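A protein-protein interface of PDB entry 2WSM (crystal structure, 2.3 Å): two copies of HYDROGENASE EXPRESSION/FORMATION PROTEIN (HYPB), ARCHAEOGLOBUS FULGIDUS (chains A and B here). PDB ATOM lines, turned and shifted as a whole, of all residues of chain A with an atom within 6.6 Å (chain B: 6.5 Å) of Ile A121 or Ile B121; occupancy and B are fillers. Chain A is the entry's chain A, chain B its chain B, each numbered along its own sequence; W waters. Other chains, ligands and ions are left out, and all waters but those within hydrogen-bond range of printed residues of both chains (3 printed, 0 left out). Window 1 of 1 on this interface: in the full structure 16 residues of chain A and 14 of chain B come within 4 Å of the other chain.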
ATOM      1  N   CYS A  92      -7.212 -32.726   8.227  1.00  0.00           N
ATOM      2  CA  CYS A  92      -6.191 -31.690   8.097  1.00  0.00           C
ATOM      3  C   CYS A  92      -4.806 -32.235   8.428  1.00  0.00           C
ATOM      4  O   CYS A  92      -3.933 -31.492   8.857  1.00  0.00           O
ATOM      5  CB  CYS A  92      -6.515 -30.519   9.030  1.00  0.00           C
ATOM      6  SG  CYS A  92      -6.824 -31.003  10.763  1.00  0.00           S
ATOM      7  N   HIS A  93      -4.613 -33.539   8.232  1.00  0.00           N
ATOM      8  CA  HIS A  93      -3.363 -34.202   8.601  1.00  0.00           C
ATOM      9  C   HIS A  93      -3.390 -35.646   8.111  1.00  0.00           C
ATOM     10  O   HIS A  93      -4.457 -36.215   7.948  1.00  0.00           O
ATOM     11  CB  HIS A  93      -3.246 -34.235  10.122  1.00  0.00           C
ATOM     12  CG  HIS A  93      -4.293 -35.087  10.769  1.00  0.00           C
ATOM     13  ND1 HIS A  93      -4.146 -36.448  10.935  1.00  0.00           N
ATOM     14  CD2 HIS A  93      -5.522 -34.782  11.248  1.00  0.00           C
ATOM     15  CE1 HIS A  93      -5.228 -36.939  11.511  1.00  0.00           C
ATOM     16  NE2 HIS A  93      -6.079 -35.950  11.708  1.00  0.00           N
ATOM     17  N   ASN A 119      -0.191 -27.821   6.588  1.00  0.00           N
ATOM     18  CA  ASN A 119      -0.807 -27.396   7.843  1.00  0.00           C
ATOM     19  C   ASN A 119       0.192 -27.481   8.997  1.00  0.00           C
ATOM     20  O   ASN A 119       0.941 -28.448   9.098  1.00  0.00           O
ATOM     21  CB  ASN A 119      -2.046 -28.264   8.116  1.00  0.00           C
ATOM     22  CG  ASN A 119      -2.644 -28.025   9.481  1.00  0.00           C
ATOM     23  OD1 ASN A 119      -2.239 -28.640  10.459  1.00  0.00           O
ATOM     24  ND2 ASN A 119      -3.638 -27.147   9.551  1.00  0.00           N
ATOM     25  N   LEU A 120       0.205 -26.473   9.865  1.00  0.00           N
ATOM     26  CA  LEU A 120       1.187 -26.404  10.947  1.00  0.00           C
ATOM     27  C   LEU A 120       0.633 -26.754  12.320  1.00  0.00           C
ATOM     28  O   LEU A 120       1.297 -26.539  13.335  1.00  0.00           O
ATOM     29  CB  LEU A 120       1.830 -25.016  11.004  1.00  0.00           C
ATOM     30  CG  LEU A 120       2.828 -24.722   9.880  1.00  0.00           C
ATOM     31  CD1 LEU A 120       3.481 -23.367  10.066  1.00  0.00           C
ATOM     32  CD2 LEU A 120       3.868 -25.817   9.807  1.00  0.00           C
ATOM     33  N   ILE A 121      -0.576 -27.297  12.355  1.00  0.00           N
ATOM     34  CA  ILE A 121      -1.244 -27.569  13.627  1.00  0.00           C
ATOM     35  C   ILE A 121      -1.634 -29.048  13.785  1.00  0.00           C
ATOM     36  O   ILE A 121      -1.102 -29.753  14.641  1.00  0.00           O
ATOM     37  CB  ILE A 121      -2.510 -26.681  13.787  1.00  0.00           C
ATOM     38  CG1 ILE A 121      -2.128 -25.259  14.197  1.00  0.00           C
ATOM     39  CG2 ILE A 121      -3.477 -27.268  14.805  1.00  0.00           C
ATOM     40  CD1 ILE A 121      -2.121 -24.277  13.054  1.00  0.00           C
ATOM     41  N   CYS A 122      -2.559 -29.504  12.946  1.00  0.00           N
ATOM     42  CA  CYS A 122      -3.163 -30.831  13.076  1.00  0.00           C
ATOM     43  C   CYS A 122      -2.192 -32.017  13.153  1.00  0.00           C
ATOM     44  O   CYS A 122      -2.435 -32.950  13.909  1.00  0.00           O
ATOM     45  CB  CYS A 122      -4.191 -31.063  11.956  1.00  0.00           C
ATOM     46  SG  CYS A 122      -5.590 -29.890  11.941  1.00  0.00           S
ATOM     47  N   PRO A 123      -1.103 -32.001  12.358  1.00  0.00           N
ATOM     48  CA  PRO A 123      -0.191 -33.156  12.323  1.00  0.00           C
ATOM     49  C   PRO A 123       0.544 -33.451  13.643  1.00  0.00           C
ATOM     50  O   PRO A 123       1.111 -34.532  13.788  1.00  0.00           O
ATOM     51  CB  PRO A 123       0.822 -32.770  11.238  1.00  0.00           C
ATOM     52  CG  PRO A 123       0.084 -31.809  10.359  1.00  0.00           C
ATOM     53  CD  PRO A 123      -0.751 -31.008  11.328  1.00  0.00           C
ATOM     54  N   VAL A 124       0.533 -32.511  14.581  1.00  0.00           N
ATOM     55  CA  VAL A 124       1.279 -32.676  15.826  1.00  0.00           C
ATOM     56  C   VAL A 124       1.043 -34.035  16.488  1.00  0.00           C
ATOM     57  O   VAL A 124       1.993 -34.754  16.775  1.00  0.00           O
ATOM     58  CB  VAL A 124       0.964 -31.550  16.826  1.00  0.00           C
ATOM     59  CG1 VAL A 124       1.459 -31.912  18.223  1.00  0.00           C
ATOM     60  CG2 VAL A 124       1.578 -30.243  16.355  1.00  0.00           C
ATOM     61  N   ASP A 125      -0.224 -34.389  16.698  1.00  0.00           N
ATOM     62  CA  ASP A 125      -0.582 -35.559  17.502  1.00  0.00           C
ATOM     63  C   ASP A 125      -0.667 -36.886  16.755  1.00  0.00           C
ATOM     64  O   ASP A 125      -1.053 -37.896  17.343  1.00  0.00           O
ATOM     65  CB  ASP A 125      -1.922 -35.327  18.201  1.00  0.00           C
ATOM     66  CG  ASP A 125      -1.819 -34.349  19.346  1.00  0.00           C
ATOM     67  OD1 ASP A 125      -2.766 -33.557  19.517  1.00  0.00           O
ATOM     68  OD2 ASP A 125      -0.795 -34.370  20.072  1.00  0.00           O
ATOM     69  N   PHE A 126      -0.323 -36.899  15.472  1.00  0.00           N
ATOM     70  CA  PHE A 126      -0.459 -38.124  14.699  1.00  0.00           C
ATOM     71  C   PHE A 126       0.855 -38.808  14.313  1.00  0.00           C
ATOM     72  O   PHE A 126       1.550 -38.402  13.384  1.00  0.00           O
ATOM     73  CB  PHE A 126      -1.378 -37.893  13.503  1.00  0.00           C
ATOM     74  CG  PHE A 126      -2.750 -37.440  13.904  1.00  0.00           C
ATOM     75  CD1 PHE A 126      -3.720 -38.365  14.256  1.00  0.00           C
ATOM     76  CD2 PHE A 126      -3.054 -36.089  13.987  1.00  0.00           C
ATOM     77  CE1 PHE A 126      -4.985 -37.951  14.649  1.00  0.00           C
ATOM     78  CE2 PHE A 126      -4.310 -35.668  14.379  1.00  0.00           C
ATOM     79  CZ  PHE A 126      -5.281 -36.600  14.711  1.00  0.00           C
ATOM     80  N   HIS A 149       4.000 -21.390  16.416  1.00  0.00           N
ATOM     81  CA  HIS A 149       3.664 -22.818  16.301  1.00  0.00           C
ATOM     82  C   HIS A 149       4.622 -23.732  17.055  1.00  0.00           C
ATOM     83  O   HIS A 149       5.300 -24.566  16.459  1.00  0.00           O
ATOM     84  CB  HIS A 149       3.580 -23.233  14.823  1.00  0.00           C
ATOM     85  CG  HIS A 149       2.556 -22.465  14.051  1.00  0.00           C
ATOM     86  ND1 HIS A 149       2.878 -21.383  13.264  1.00  0.00           N
ATOM     87  CD2 HIS A 149       1.209 -22.591  13.987  1.00  0.00           C
ATOM     88  CE1 HIS A 149       1.776 -20.890  12.725  1.00  0.00           C
ATOM     89  NE2 HIS A 149       0.748 -21.603  13.152  1.00  0.00           N
ATOM     90  N   GLU A 151       4.021 -26.253  19.073  1.00  0.00           N
ATOM     91  CA  GLU A 151       3.665 -27.668  19.145  1.00  0.00           C
ATOM     92  C   GLU A 151       4.303 -28.481  18.022  1.00  0.00           C
ATOM     93  O   GLU A 151       4.901 -29.531  18.267  1.00  0.00           O
ATOM     94  CB  GLU A 151       2.143 -27.876  19.129  1.00  0.00           C
ATOM     95  CG  GLU A 151       1.398 -27.359  20.353  1.00  0.00           C
ATOM     96  CD  GLU A 151       0.709 -26.026  20.111  1.00  0.00           C
ATOM     97  OE1 GLU A 151      -0.459 -25.894  20.530  1.00  0.00           O
ATOM     98  OE2 GLU A 151       1.316 -25.117  19.496  1.00  0.00           O
ATOM     99  N   ILE A 152       4.179 -27.996  16.789  1.00  0.00           N
ATOM    100  CA  ILE A 152       4.713 -28.737  15.665  1.00  0.00           C
ATOM    101  C   ILE A 152       6.234 -28.672  15.612  1.00  0.00           C
ATOM    102  O   ILE A 152       6.884 -29.660  15.262  1.00  0.00           O
ATOM    103  CB  ILE A 152       4.095 -28.310  14.320  1.00  0.00           C
ATOM    104  CG1 ILE A 152       4.400 -29.363  13.248  1.00  0.00           C
ATOM    105  CG2 ILE A 152       4.593 -26.940  13.895  1.00  0.00           C
ATOM    106  CD1 ILE A 152       3.382 -29.403  12.113  1.00  0.00           C
ATOM    107  N   CYS B  92     -10.382 -34.751  13.613  1.00  0.00           N
ATOM    108  CA  CYS B  92      -9.999 -34.501  15.008  1.00  0.00           C
ATOM    109  C   CYS B  92     -10.556 -33.182  15.541  1.00  0.00           C
ATOM    110  O   CYS B  92     -10.051 -32.628  16.515  1.00  0.00           O
ATOM    111  CB  CYS B  92      -8.476 -34.507  15.151  1.00  0.00           C
ATOM    112  SG  CYS B  92      -7.578 -33.408  13.992  1.00  0.00           S
ATOM    113  N   ASN B 119      -9.642 -32.097  22.526  1.00  0.00           N
ATOM    114  CA  ASN B 119      -8.458 -31.904  21.707  1.00  0.00           C
ATOM    115  C   ASN B 119      -8.054 -30.431  21.705  1.00  0.00           C
ATOM    116  O   ASN B 119      -8.871 -29.566  21.399  1.00  0.00           O
ATOM    117  CB  ASN B 119      -8.800 -32.367  20.288  1.00  0.00           C
ATOM    118  CG  ASN B 119      -7.628 -32.322  19.349  1.00  0.00           C
ATOM    119  OD1 ASN B 119      -7.072 -31.260  19.073  1.00  0.00           O
ATOM    120  ND2 ASN B 119      -7.262 -33.480  18.815  1.00  0.00           N
ATOM    121  N   LEU B 120      -6.797 -30.148  22.041  1.00  0.00           N
ATOM    122  CA  LEU B 120      -6.329 -28.766  22.170  1.00  0.00           C
ATOM    123  C   LEU B 120      -5.576 -28.238  20.953  1.00  0.00           C
ATOM    124  O   LEU B 120      -4.944 -27.175  21.010  1.00  0.00           O
ATOM    125  CB  LEU B 120      -5.453 -28.618  23.419  1.00  0.00           C
ATOM    126  CG  LEU B 120      -6.214 -28.771  24.739  1.00  0.00           C
ATOM    127  CD1 LEU B 120      -5.270 -28.924  25.922  1.00  0.00           C
ATOM    128  CD2 LEU B 120      -7.152 -27.588  24.932  1.00  0.00           C
ATOM    129  N   ILE B 121      -5.655 -28.966  19.848  1.00  0.00           N
ATOM    130  CA  ILE B 121      -4.834 -28.651  18.687  1.00  0.00           C
ATOM    131  C   ILE B 121      -5.633 -28.419  17.394  1.00  0.00           C
ATOM    132  O   ILE B 121      -5.689 -27.294  16.895  1.00  0.00           O
ATOM    133  CB  ILE B 121      -3.721 -29.715  18.518  1.00  0.00           C
ATOM    134  CG1 ILE B 121      -2.569 -29.394  19.476  1.00  0.00           C
ATOM    135  CG2 ILE B 121      -3.232 -29.792  17.078  1.00  0.00           C
ATOM    136  CD1 ILE B 121      -1.818 -30.603  19.963  1.00  0.00           C
ATOM    137  N   CYS B 122      -6.270 -29.470  16.885  1.00  0.00           N
ATOM    138  CA  CYS B 122      -7.002 -29.412  15.614  1.00  0.00           C
ATOM    139  C   CYS B 122      -8.012 -28.270  15.437  1.00  0.00           C
ATOM    140  O   CYS B 122      -8.053 -27.654  14.376  1.00  0.00           O
ATOM    141  CB  CYS B 122      -7.692 -30.749  15.338  1.00  0.00           C
ATOM    142  SG  CYS B 122      -6.555 -32.126  15.209  1.00  0.00           S
ATOM    143  N   PRO B 123      -8.837 -27.996  16.467  1.00  0.00           N
ATOM    144  CA  PRO B 123      -9.924 -27.015  16.331  1.00  0.00           C
ATOM    145  C   PRO B 123      -9.449 -25.588  16.063  1.00  0.00           C
ATOM    146  O   PRO B 123     -10.252 -24.742  15.671  1.00  0.00           O
ATOM    147  CB  PRO B 123     -10.626 -27.073  17.696  1.00  0.00           C
ATOM    148  CG  PRO B 123     -10.209 -28.364  18.301  1.00  0.00           C
ATOM    149  CD  PRO B 123      -8.813 -28.601  17.808  1.00  0.00           C
ATOM    150  N   VAL B 124      -8.161 -25.332  16.275  1.00  0.00           N
ATOM    151  CA  VAL B 124      -7.601 -23.989  16.151  1.00  0.00           C
ATOM    152  C   VAL B 124      -7.944 -23.286  14.846  1.00  0.00           C
ATOM    153  O   VAL B 124      -8.342 -22.125  14.855  1.00  0.00           O
ATOM    154  CB  VAL B 124      -6.076 -24.014  16.321  1.00  0.00           C
ATOM    155  CG1 VAL B 124      -5.451 -22.750  15.750  1.00  0.00           C
ATOM    156  CG2 VAL B 124      -5.718 -24.183  17.794  1.00  0.00           C
ATOM    157  N   ASP B 125      -7.793 -23.989  13.728  1.00  0.00           N
ATOM    158  CA  ASP B 125      -7.951 -23.379  12.409  1.00  0.00           C
ATOM    159  C   ASP B 125      -9.399 -23.256  11.952  1.00  0.00           C
ATOM    160  O   ASP B 125      -9.703 -22.484  11.044  1.00  0.00           O
ATOM    161  CB  ASP B 125      -7.181 -24.179  11.359  1.00  0.00           C
ATOM    162  CG  ASP B 125      -5.703 -23.873  11.361  1.00  0.00           C
ATOM    163  OD1 ASP B 125      -4.920 -24.739  10.916  1.00  0.00           O
ATOM    164  OD2 ASP B 125      -5.329 -22.769  11.806  1.00  0.00           O
ATOM    165  N   HIS B 149       0.131 -24.905  24.672  1.00  0.00           N
ATOM    166  CA  HIS B 149      -0.902 -24.807  23.645  1.00  0.00           C
ATOM    167  C   HIS B 149      -1.361 -23.382  23.398  1.00  0.00           C
ATOM    168  O   HIS B 149      -2.545 -23.088  23.492  1.00  0.00           O
ATOM    169  CB  HIS B 149      -2.101 -25.668  24.025  1.00  0.00           C
ATOM    170  CG  HIS B 149      -1.761 -27.104  24.260  1.00  0.00           C
ATOM    171  ND1 HIS B 149      -1.756 -27.672  25.514  1.00  0.00           N
ATOM    172  CD2 HIS B 149      -1.409 -28.088  23.400  1.00  0.00           C
ATOM    173  CE1 HIS B 149      -1.422 -28.947  25.418  1.00  0.00           C
ATOM    174  NE2 HIS B 149      -1.210 -29.225  24.145  1.00  0.00           N
ATOM    175  N   GLU B 151      -1.640 -21.655  20.636  1.00  0.00           N
ATOM    176  CA  GLU B 151      -2.461 -21.430  19.453  1.00  0.00           C
ATOM    177  C   GLU B 151      -3.956 -21.442  19.770  1.00  0.00           C
ATOM    178  O   GLU B 151      -4.692 -20.542  19.362  1.00  0.00           O
ATOM    179  CB  GLU B 151      -2.112 -22.460  18.381  1.00  0.00           C
ATOM    180  CG  GLU B 151      -0.651 -22.872  18.465  1.00  0.00           C
ATOM    181  CD  GLU B 151      -0.118 -23.411  17.175  1.00  0.00           C
ATOM    182  OE1 GLU B 151      -0.602 -22.977  16.108  1.00  0.00           O
ATOM    183  OE2 GLU B 151       0.788 -24.268  17.228  1.00  0.00           O
ATOM    184  N   ILE B 152      -4.408 -22.450  20.505  1.00  0.00           N
ATOM    185  CA  ILE B 152      -5.830 -22.534  20.818  1.00  0.00           C
ATOM    186  C   ILE B 152      -6.255 -21.513  21.884  1.00  0.00           C
ATOM    187  O   ILE B 152      -7.315 -20.890  21.775  1.00  0.00           O
ATOM    188  CB  ILE B 152      -6.267 -23.974  21.192  1.00  0.00           C
ATOM    189  CG1 ILE B 152      -7.795 -24.104  21.110  1.00  0.00           C
ATOM    190  CG2 ILE B 152      -5.746 -24.367  22.565  1.00  0.00           C
ATOM    191  CD1 ILE B 152      -8.298 -25.543  21.177  1.00  0.00           C
HETATM  192  O   HOH W   1       2.056 -26.229  16.100  1.00  0.00           O
HETATM  193  O   HOH W   2      -4.697 -33.874  18.102  1.00  0.00           O
HETATM  194  O   HOH W   3      -3.102 -25.241  20.735  1.00  0.00           O
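Water W2 bridges OD1 of Asp A125 and ND2 of Asn B119. Water W1 lies within hydrogen-bond range of the side-chain carboxylate of Glu B151 (2.6 Å), the backbone NH of Ile A152 (2.8 Å) and the backbone carbonyl oxygen of Leu A120 (2.9 Å). Water W3 lies within hydrogen-bond range of O of Leu B120 (2.7 Å), OE1 of Glu A151 (2.7 Å) and N of Ile B152 (3.1 Å).
Of the 13 printed residues of chain A, 9 touch a printed residue of chain B. Along chain A the printed residues that touch a printed residue of chain B span positions 93 to 151.
The side-chain sulfur (SG) of Cys B92 forms a disulfide with the side-chain sulfur (SG) of Cys B122, 2.0 Å away. OD1 of Asn B119 is in hydrogen-bond range of N of Ile B121, at 2.8 Å. The backbone NH (N) of Ile A121 is in hydrogen-bond range of the side-chain amide oxygen (OD1) of Asn A119. The side-chain sulfur of Cys A122 is disulfide-bonded to the side-chain sulfur of Cys A92, 2.0 Å away. The backbone NH (N) of Cys A122 sits at hydrogen-bond distance from the side-chain amide oxygen (OD1) of Asn A119 (2.7 Å). OD1 of Asn B119 is in hydrogen-bond range of N of Cys B122.
Printed residues of chain A within 4 Å of Ile B121: Ile A121 (3.0 Å), Val A124 (3.9 Å) and Asp A125 (3.1 Å). Printed residues of chain A within 4 Å of Asp B125: Asn A119 and Ile A121. Of the printed residues of chain B, His A93 touches Cys B92. Of the printed residues of chain A, Cys B92 touches His A93 and Phe A126. Leu A120 touches none of the printed residues of chain B. The nearest printed residue of chain A that does not touch Asp B125 is Cys A122 (5.3 Å).
Among the printed residues, pairs that only touch across the chains: His A149 with Glu B151 (2.8 Å), Ile A121 with Ile B121 (3.0 Å), Asp A125 with Ile B121 (3.1 Å), Glu A151 with His B149 (3.3 Å), Ile A121 with Glu B151 (3.3 Å), Ile A121 with Asp B125 (3.6 Å), Phe A126 with Cys B92 (3.8 Å), Val A124 with Ile B121 (3.9 Å) and Cys A122 with Cys B122 (3.96 Å).
The side-chain amide nitrogen (ND2) of Asn A119 sits at hydrogen-bond distance from the side-chain carboxylate (OD1) of Asp B125, at 3.1 Å. A ring nitrogen (NE2) of His A93 lies close to the side-chain sulfur (SG) of Cys B92 (3.7 Å). The side-chain carboxylate of Glu A151 sits close to the side-chain carboxylate of Glu B151, 2.5 Å away.
Ile B121 touches its own counterpart, Ile A121. Cys B122 touches its own counterpart, Cys A122. Val A124 touches Ile B121, but with the chains exchanged Ile A121 does not touch Val B124 (4.4 Å). Glu A151 touches its own counterpart, Glu B151. 11 positions are printed for both chains.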
